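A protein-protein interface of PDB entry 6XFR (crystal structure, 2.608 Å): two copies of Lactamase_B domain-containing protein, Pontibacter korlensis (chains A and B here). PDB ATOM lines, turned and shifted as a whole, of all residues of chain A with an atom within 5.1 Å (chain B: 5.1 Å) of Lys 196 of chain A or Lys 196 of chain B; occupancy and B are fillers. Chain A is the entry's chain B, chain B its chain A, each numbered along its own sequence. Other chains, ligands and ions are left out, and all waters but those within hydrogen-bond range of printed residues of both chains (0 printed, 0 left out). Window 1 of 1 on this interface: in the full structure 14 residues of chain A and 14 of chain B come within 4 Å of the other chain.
Among the printed residues, pairs that only touch across the chains: Lys 196 of chain A with Lys 196 of chain B.
The backbone carbonyl oxygen of Lys 154 of chain B sits at hydrogen-bond distance from the backbone NH of Lys 196 of chain B, 2.8 Å away.
The backbone NH of Lys 196 of chain A lies within hydrogen-bond range of the backbone carbonyl oxygen of Lys 154 of chain A, at 2.8 Å.
Of the printed residues of chain B, Lys 196 of chain A touches Lys 196 and Gln 208.
Val 198 of chain A touches none of the printed residues of chain B.
Printed residues of chain B within 4 Å of Gln 208 of chain A: Lys 196.
Ile 155 of chain B touches none of the printed residues of chain A.
Of chain A, only Lys 196 and Gln 208 come within 4 Å of Lys 196 of chain B.
Of the printed residues of chain A, Gln 208 of chain B touches Lys 196 (3.1 Å).
The nearest printed residue of chain A that does not touch Gln 208 of chain B is Gln 153 of chain A (6.2 Å).
Lys 196 of chain B touches its own counterpart, Lys 196 of chain A.
Lys 196 of chain A touches Gln 208 of chain B, and with the chains exchanged Gln 208 of chain A touches Lys 196 of chain B.
Positions printed for both chains: 153, 154, 155, 194, 195, 196, 197, 198, 206, 207 and 208.
Of the 11 printed residues of chain B, 2 touch a printed residue of chain A.
Among the printed residues, 3 pairs touch across the chains.
Among the printed residues, no Asp or Glu carboxylate lies within 4 Å of a Lys or Arg side-chain nitrogen of the other chain.
OE1 of Gln 208 of chain A sits at hydrogen-bond distance from NZ of Lys 196 of chain B, at 3.0 Å.
The side-chain amide nitrogen of Gln 208 of chain B lies close to the side-chain amino group of Lys 196 of chain A.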
ATOM      1  N   GLN A 153      -8.341   6.772  21.896  1.00  0.00           N
ATOM      2  CA  GLN A 153      -9.023   8.046  22.050  1.00  0.00           C
ATOM      3  C   GLN A 153      -9.445   8.653  20.712  1.00  0.00           C
ATOM      4  O   GLN A 153     -10.198   9.636  20.706  1.00  0.00           O
ATOM      5  CB  GLN A 153      -8.120   9.029  22.815  1.00  0.00           C
ATOM      6  CG  GLN A 153      -7.807   8.640  24.242  1.00  0.00           C
ATOM      7  CD  GLN A 153      -6.518   7.808  24.374  1.00  0.00           C
ATOM      8  OE1 GLN A 153      -6.122   7.108  23.443  1.00  0.00           O
ATOM      9  NE2 GLN A 153      -5.872   7.879  25.544  1.00  0.00           N
ATOM     10  N   LYS A 154      -9.029   8.046  19.595  1.00  0.00           N
ATOM     11  CA  LYS A 154      -9.241   8.551  18.229  1.00  0.00           C
ATOM     12  C   LYS A 154      -8.805  10.013  18.084  1.00  0.00           C
ATOM     13  O   LYS A 154      -9.523  10.863  17.550  1.00  0.00           O
ATOM     14  CB  LYS A 154     -10.696   8.357  17.796  1.00  0.00           C
ATOM     15  CG  LYS A 154     -11.203   6.942  18.007  1.00  0.00           C
ATOM     16  CD  LYS A 154     -11.946   6.442  16.790  1.00  0.00           C
ATOM     17  CE  LYS A 154     -12.221   4.973  16.904  1.00  0.00           C
ATOM     18  NZ  LYS A 154     -13.633   4.798  17.356  1.00  0.00           N
ATOM     19  N   ILE A 155      -7.579  10.283  18.512  1.00  0.00           N
ATOM     20  CA  ILE A 155      -6.971  11.601  18.462  1.00  0.00           C
ATOM     21  C   ILE A 155      -5.814  11.557  17.466  1.00  0.00           C
ATOM     22  O   ILE A 155      -4.900  10.731  17.602  1.00  0.00           O
ATOM     23  CB  ILE A 155      -6.469  12.016  19.852  1.00  0.00           C
ATOM     24  CG1 ILE A 155      -7.641  12.202  20.822  1.00  0.00           C
ATOM     25  CG2 ILE A 155      -5.614  13.291  19.753  1.00  0.00           C
ATOM     26  CD1 ILE A 155      -7.267  12.881  22.154  1.00  0.00           C
ATOM     27  N   LYS A 194     -12.219   7.735  11.183  1.00  0.00           N
ATOM     28  CA  LYS A 194     -13.001   7.946  12.400  1.00  0.00           C
ATOM     29  C   LYS A 194     -12.215   8.713  13.463  1.00  0.00           C
ATOM     30  O   LYS A 194     -12.433   8.518  14.658  1.00  0.00           O
ATOM     31  CB  LYS A 194     -13.509   6.615  12.966  1.00  0.00           C
ATOM     32  CG  LYS A 194     -14.492   5.936  12.000  1.00  0.00           C
ATOM     33  CD  LYS A 194     -15.990   5.880  12.407  1.00  0.00           C
ATOM     34  CE  LYS A 194     -16.795   4.910  11.528  1.00  0.00           C
ATOM     35  NZ  LYS A 194     -17.186   3.575  11.970  1.00  0.00           N
ATOM     36  N   ALA A 195     -11.292   9.579  13.047  1.00  0.00           N
ATOM     37  CA  ALA A 195     -10.628  10.472  13.992  1.00  0.00           C
ATOM     38  C   ALA A 195     -11.596  11.523  14.552  1.00  0.00           C
ATOM     39  O   ALA A 195     -12.344  12.167  13.811  1.00  0.00           O
ATOM     40  CB  ALA A 195      -9.445  11.149  13.314  1.00  0.00           C
ATOM     41  N   LYS A 196     -11.563  11.720  15.864  1.00  0.00           N
ATOM     42  CA  LYS A 196     -12.477  12.674  16.487  1.00  0.00           C
ATOM     43  C   LYS A 196     -11.850  14.044  16.673  1.00  0.00           C
ATOM     44  O   LYS A 196     -12.513  15.058  16.469  1.00  0.00           O
ATOM     45  CB  LYS A 196     -12.952  12.152  17.841  1.00  0.00           C
ATOM     46  CG  LYS A 196     -13.750  10.880  17.792  1.00  0.00           C
ATOM     47  CD  LYS A 196     -14.578  10.743  19.036  1.00  0.00           C
ATOM     48  CE  LYS A 196     -13.870  10.056  20.180  1.00  0.00           C
ATOM     49  NZ  LYS A 196     -14.704  10.148  21.431  1.00  0.00           N
ATOM     50  N   VAL A 197     -10.587  14.103  17.066  1.00  0.00           N
ATOM     51  CA  VAL A 197      -9.849  15.352  17.245  1.00  0.00           C
ATOM     52  C   VAL A 197      -8.629  15.303  16.334  1.00  0.00           C
ATOM     53  O   VAL A 197      -7.987  14.249  16.213  1.00  0.00           O
ATOM     54  CB  VAL A 197      -9.389  15.585  18.704  1.00  0.00           C
ATOM     55  CG1 VAL A 197      -8.896  17.021  18.892  1.00  0.00           C
ATOM     56  CG2 VAL A 197     -10.461  15.243  19.698  1.00  0.00           C
ATOM     57  N   VAL A 198      -8.330  16.436  15.684  1.00  0.00           N
ATOM     58  CA  VAL A 198      -7.120  16.627  14.878  1.00  0.00           C
ATOM     59  C   VAL A 198      -6.357  17.831  15.420  1.00  0.00           C
ATOM     60  O   VAL A 198      -6.906  18.942  15.474  1.00  0.00           O
ATOM     61  CB  VAL A 198      -7.465  16.818  13.399  1.00  0.00           C
ATOM     62  CG1 VAL A 198      -6.195  17.170  12.579  1.00  0.00           C
ATOM     63  CG2 VAL A 198      -8.206  15.565  12.881  1.00  0.00           C
ATOM     64  N   GLY A 206      -9.513  20.904  16.025  1.00  0.00           N
ATOM     65  CA  GLY A 206     -10.904  20.739  15.636  1.00  0.00           C
ATOM     66  C   GLY A 206     -11.222  19.314  15.243  1.00  0.00           C
ATOM     67  O   GLY A 206     -10.555  18.373  15.657  1.00  0.00           O
ATOM     68  N   ASP A 207     -12.250  19.153  14.419  1.00  0.00           N
ATOM     69  CA  ASP A 207     -12.564  17.816  13.937  1.00  0.00           C
ATOM     70  C   ASP A 207     -11.845  17.581  12.610  1.00  0.00           C
ATOM     71  O   ASP A 207     -10.842  18.227  12.299  1.00  0.00           O
ATOM     72  CB  ASP A 207     -14.080  17.599  13.866  1.00  0.00           C
ATOM     73  CG  ASP A 207     -14.811  18.610  12.987  1.00  0.00           C
ATOM     74  OD1 ASP A 207     -14.153  19.502  12.388  1.00  0.00           O
ATOM     75  OD2 ASP A 207     -16.083  18.490  12.913  1.00  0.00           O
ATOM     76  N   GLN A 208     -12.325  16.623  11.835  1.00  0.00           N
ATOM     77  CA  GLN A 208     -11.654  16.278  10.592  1.00  0.00           C
ATOM     78  C   GLN A 208     -11.806  17.368   9.532  1.00  0.00           C
ATOM     79  O   GLN A 208     -11.290  17.196   8.432  1.00  0.00           O
ATOM     80  CB  GLN A 208     -12.204  14.939  10.095  1.00  0.00           C
ATOM     81  CG  GLN A 208     -13.648  15.028   9.556  1.00  0.00           C
ATOM     82  CD  GLN A 208     -14.720  15.099  10.651  1.00  0.00           C
ATOM     83  OE1 GLN A 208     -14.416  15.230  11.852  1.00  0.00           O
ATOM     84  NE2 GLN A 208     -15.983  15.000  10.236  1.00  0.00           N
ATOM     85  N   GLN B 153     -22.390  17.065  12.968  1.00  0.00           N
ATOM     86  CA  GLN B 153     -21.011  17.149  13.441  1.00  0.00           C
ATOM     87  C   GLN B 153     -20.768  16.373  14.732  1.00  0.00           C
ATOM     88  O   GLN B 153     -19.641  16.372  15.225  1.00  0.00           O
ATOM     89  CB  GLN B 153     -20.607  18.611  13.647  1.00  0.00           C
ATOM     90  CG  GLN B 153     -20.635  19.427  12.383  1.00  0.00           C
ATOM     91  CD  GLN B 153     -21.945  20.187  12.191  1.00  0.00           C
ATOM     92  OE1 GLN B 153     -22.988  19.823  12.737  1.00  0.00           O
ATOM     93  NE2 GLN B 153     -21.891  21.241  11.408  1.00  0.00           N
ATOM     94  N   LYS B 154     -21.793  15.774  15.326  1.00  0.00           N
ATOM     95  CA  LYS B 154     -21.675  15.086  16.609  1.00  0.00           C
ATOM     96  C   LYS B 154     -20.951  15.954  17.637  1.00  0.00           C
ATOM     97  O   LYS B 154     -19.992  15.533  18.287  1.00  0.00           O
ATOM     98  CB  LYS B 154     -20.994  13.733  16.428  1.00  0.00           C
ATOM     99  CG  LYS B 154     -21.759  12.897  15.406  1.00  0.00           C
ATOM    100  CD  LYS B 154     -21.544  11.416  15.552  1.00  0.00           C
ATOM    101  CE  LYS B 154     -22.310  10.688  14.476  1.00  0.00           C
ATOM    102  NZ  LYS B 154     -21.782  11.038  13.125  1.00  0.00           N
ATOM    103  N   ILE B 155     -21.448  17.176  17.780  1.00  0.00           N
ATOM    104  CA  ILE B 155     -20.931  18.175  18.695  1.00  0.00           C
ATOM    105  C   ILE B 155     -22.013  18.481  19.716  1.00  0.00           C
ATOM    106  O   ILE B 155     -23.130  18.859  19.348  1.00  0.00           O
ATOM    107  CB  ILE B 155     -20.543  19.479  17.980  1.00  0.00           C
ATOM    108  CG1 ILE B 155     -19.323  19.281  17.094  1.00  0.00           C
ATOM    109  CG2 ILE B 155     -20.276  20.565  19.035  1.00  0.00           C
ATOM    110  CD1 ILE B 155     -18.945  20.519  16.329  1.00  0.00           C
ATOM    111  N   LYS B 194     -22.262   8.740  21.051  1.00  0.00           N
ATOM    112  CA  LYS B 194     -21.291   8.899  19.986  1.00  0.00           C
ATOM    113  C   LYS B 194     -20.952  10.370  19.736  1.00  0.00           C
ATOM    114  O   LYS B 194     -20.478  10.737  18.667  1.00  0.00           O
ATOM    115  CB  LYS B 194     -21.816   8.220  18.726  1.00  0.00           C
ATOM    116  CG  LYS B 194     -21.112   6.884  18.411  1.00  0.00           C
ATOM    117  CD  LYS B 194     -21.676   5.723  19.194  1.00  0.00           C
ATOM    118  CE  LYS B 194     -23.066   5.380  18.694  1.00  0.00           C
ATOM    119  NZ  LYS B 194     -23.515   4.053  19.213  1.00  0.00           N
ATOM    120  N   ALA B 195     -21.101  11.210  20.748  1.00  0.00           N
ATOM    121  CA  ALA B 195     -20.638  12.585  20.622  1.00  0.00           C
ATOM    122  C   ALA B 195     -19.118  12.616  20.465  1.00  0.00           C
ATOM    123  O   ALA B 195     -18.386  11.927  21.182  1.00  0.00           O
ATOM    124  CB  ALA B 195     -21.059  13.406  21.847  1.00  0.00           C
ATOM    125  N   LYS B 196     -18.643  13.423  19.523  1.00  0.00           N
ATOM    126  CA  LYS B 196     -17.205  13.500  19.290  1.00  0.00           C
ATOM    127  C   LYS B 196     -16.557  14.618  20.098  1.00  0.00           C
ATOM    128  O   LYS B 196     -15.455  14.435  20.623  1.00  0.00           O
ATOM    129  CB  LYS B 196     -16.894  13.696  17.801  1.00  0.00           C
ATOM    130  CG  LYS B 196     -17.364  12.575  16.933  1.00  0.00           C
ATOM    131  CD  LYS B 196     -16.689  12.603  15.568  1.00  0.00           C
ATOM    132  CE  LYS B 196     -17.317  13.620  14.661  1.00  0.00           C
ATOM    133  NZ  LYS B 196     -16.568  13.753  13.387  1.00  0.00           N
ATOM    134  N   VAL B 197     -17.215  15.775  20.184  1.00  0.00           N
ATOM    135  CA  VAL B 197     -16.726  16.935  20.915  1.00  0.00           C
ATOM    136  C   VAL B 197     -17.787  17.340  21.934  1.00  0.00           C
ATOM    137  O   VAL B 197     -18.979  17.352  21.622  1.00  0.00           O
ATOM    138  CB  VAL B 197     -16.396  18.085  19.936  1.00  0.00           C
ATOM    139  CG1 VAL B 197     -15.790  19.248  20.673  1.00  0.00           C
ATOM    140  CG2 VAL B 197     -15.466  17.564  18.841  1.00  0.00           C
ATOM    141  N   VAL B 198     -17.351  17.651  23.154  1.00  0.00           N
ATOM    142  CA  VAL B 198     -18.216  18.172  24.216  1.00  0.00           C
ATOM    143  C   VAL B 198     -17.673  19.527  24.643  1.00  0.00           C
ATOM    144  O   VAL B 198     -16.509  19.626  25.057  1.00  0.00           O
ATOM    145  CB  VAL B 198     -18.290  17.198  25.412  1.00  0.00           C
ATOM    146  CG1 VAL B 198     -19.129  17.803  26.544  1.00  0.00           C
ATOM    147  CG2 VAL B 198     -18.826  15.808  24.992  1.00  0.00           C
ATOM    148  N   GLY B 206     -13.272  19.043  25.087  1.00  0.00           N
ATOM    149  CA  GLY B 206     -12.590  17.770  24.930  1.00  0.00           C
ATOM    150  C   GLY B 206     -13.497  16.676  24.417  1.00  0.00           C
ATOM    151  O   GLY B 206     -14.489  16.927  23.733  1.00  0.00           O
ATOM    152  N   ASP B 207     -13.161  15.438  24.757  1.00  0.00           N
ATOM    153  CA  ASP B 207     -14.034  14.351  24.334  1.00  0.00           C
ATOM    154  C   ASP B 207     -15.053  14.042  25.440  1.00  0.00           C
ATOM    155  O   ASP B 207     -15.276  14.841  26.360  1.00  0.00           O
ATOM    156  CB  ASP B 207     -13.187  13.142  23.890  1.00  0.00           C
ATOM    157  CG  ASP B 207     -12.330  12.538  25.013  1.00  0.00           C
ATOM    158  OD1 ASP B 207     -12.454  12.986  26.182  1.00  0.00           O
ATOM    159  OD2 ASP B 207     -11.521  11.603  24.704  1.00  0.00           O
ATOM    160  N   GLN B 208     -15.682  12.867  25.374  1.00  0.00           N
ATOM    161  CA  GLN B 208     -16.688  12.533  26.373  1.00  0.00           C
ATOM    162  C   GLN B 208     -16.065  12.245  27.744  1.00  0.00           C
ATOM    163  O   GLN B 208     -16.788  11.925  28.694  1.00  0.00           O
ATOM    164  CB  GLN B 208     -17.543  11.361  25.866  1.00  0.00           C
ATOM    165  CG  GLN B 208     -16.892   9.989  25.953  1.00  0.00           C
ATOM    166  CD  GLN B 208     -15.901   9.716  24.831  1.00  0.00           C
ATOM    167  OE1 GLN B 208     -14.770  10.166  24.883  1.00  0.00           O
ATOM    168  NE2 GLN B 208     -16.321   8.959  23.820  1.00  0.00           N
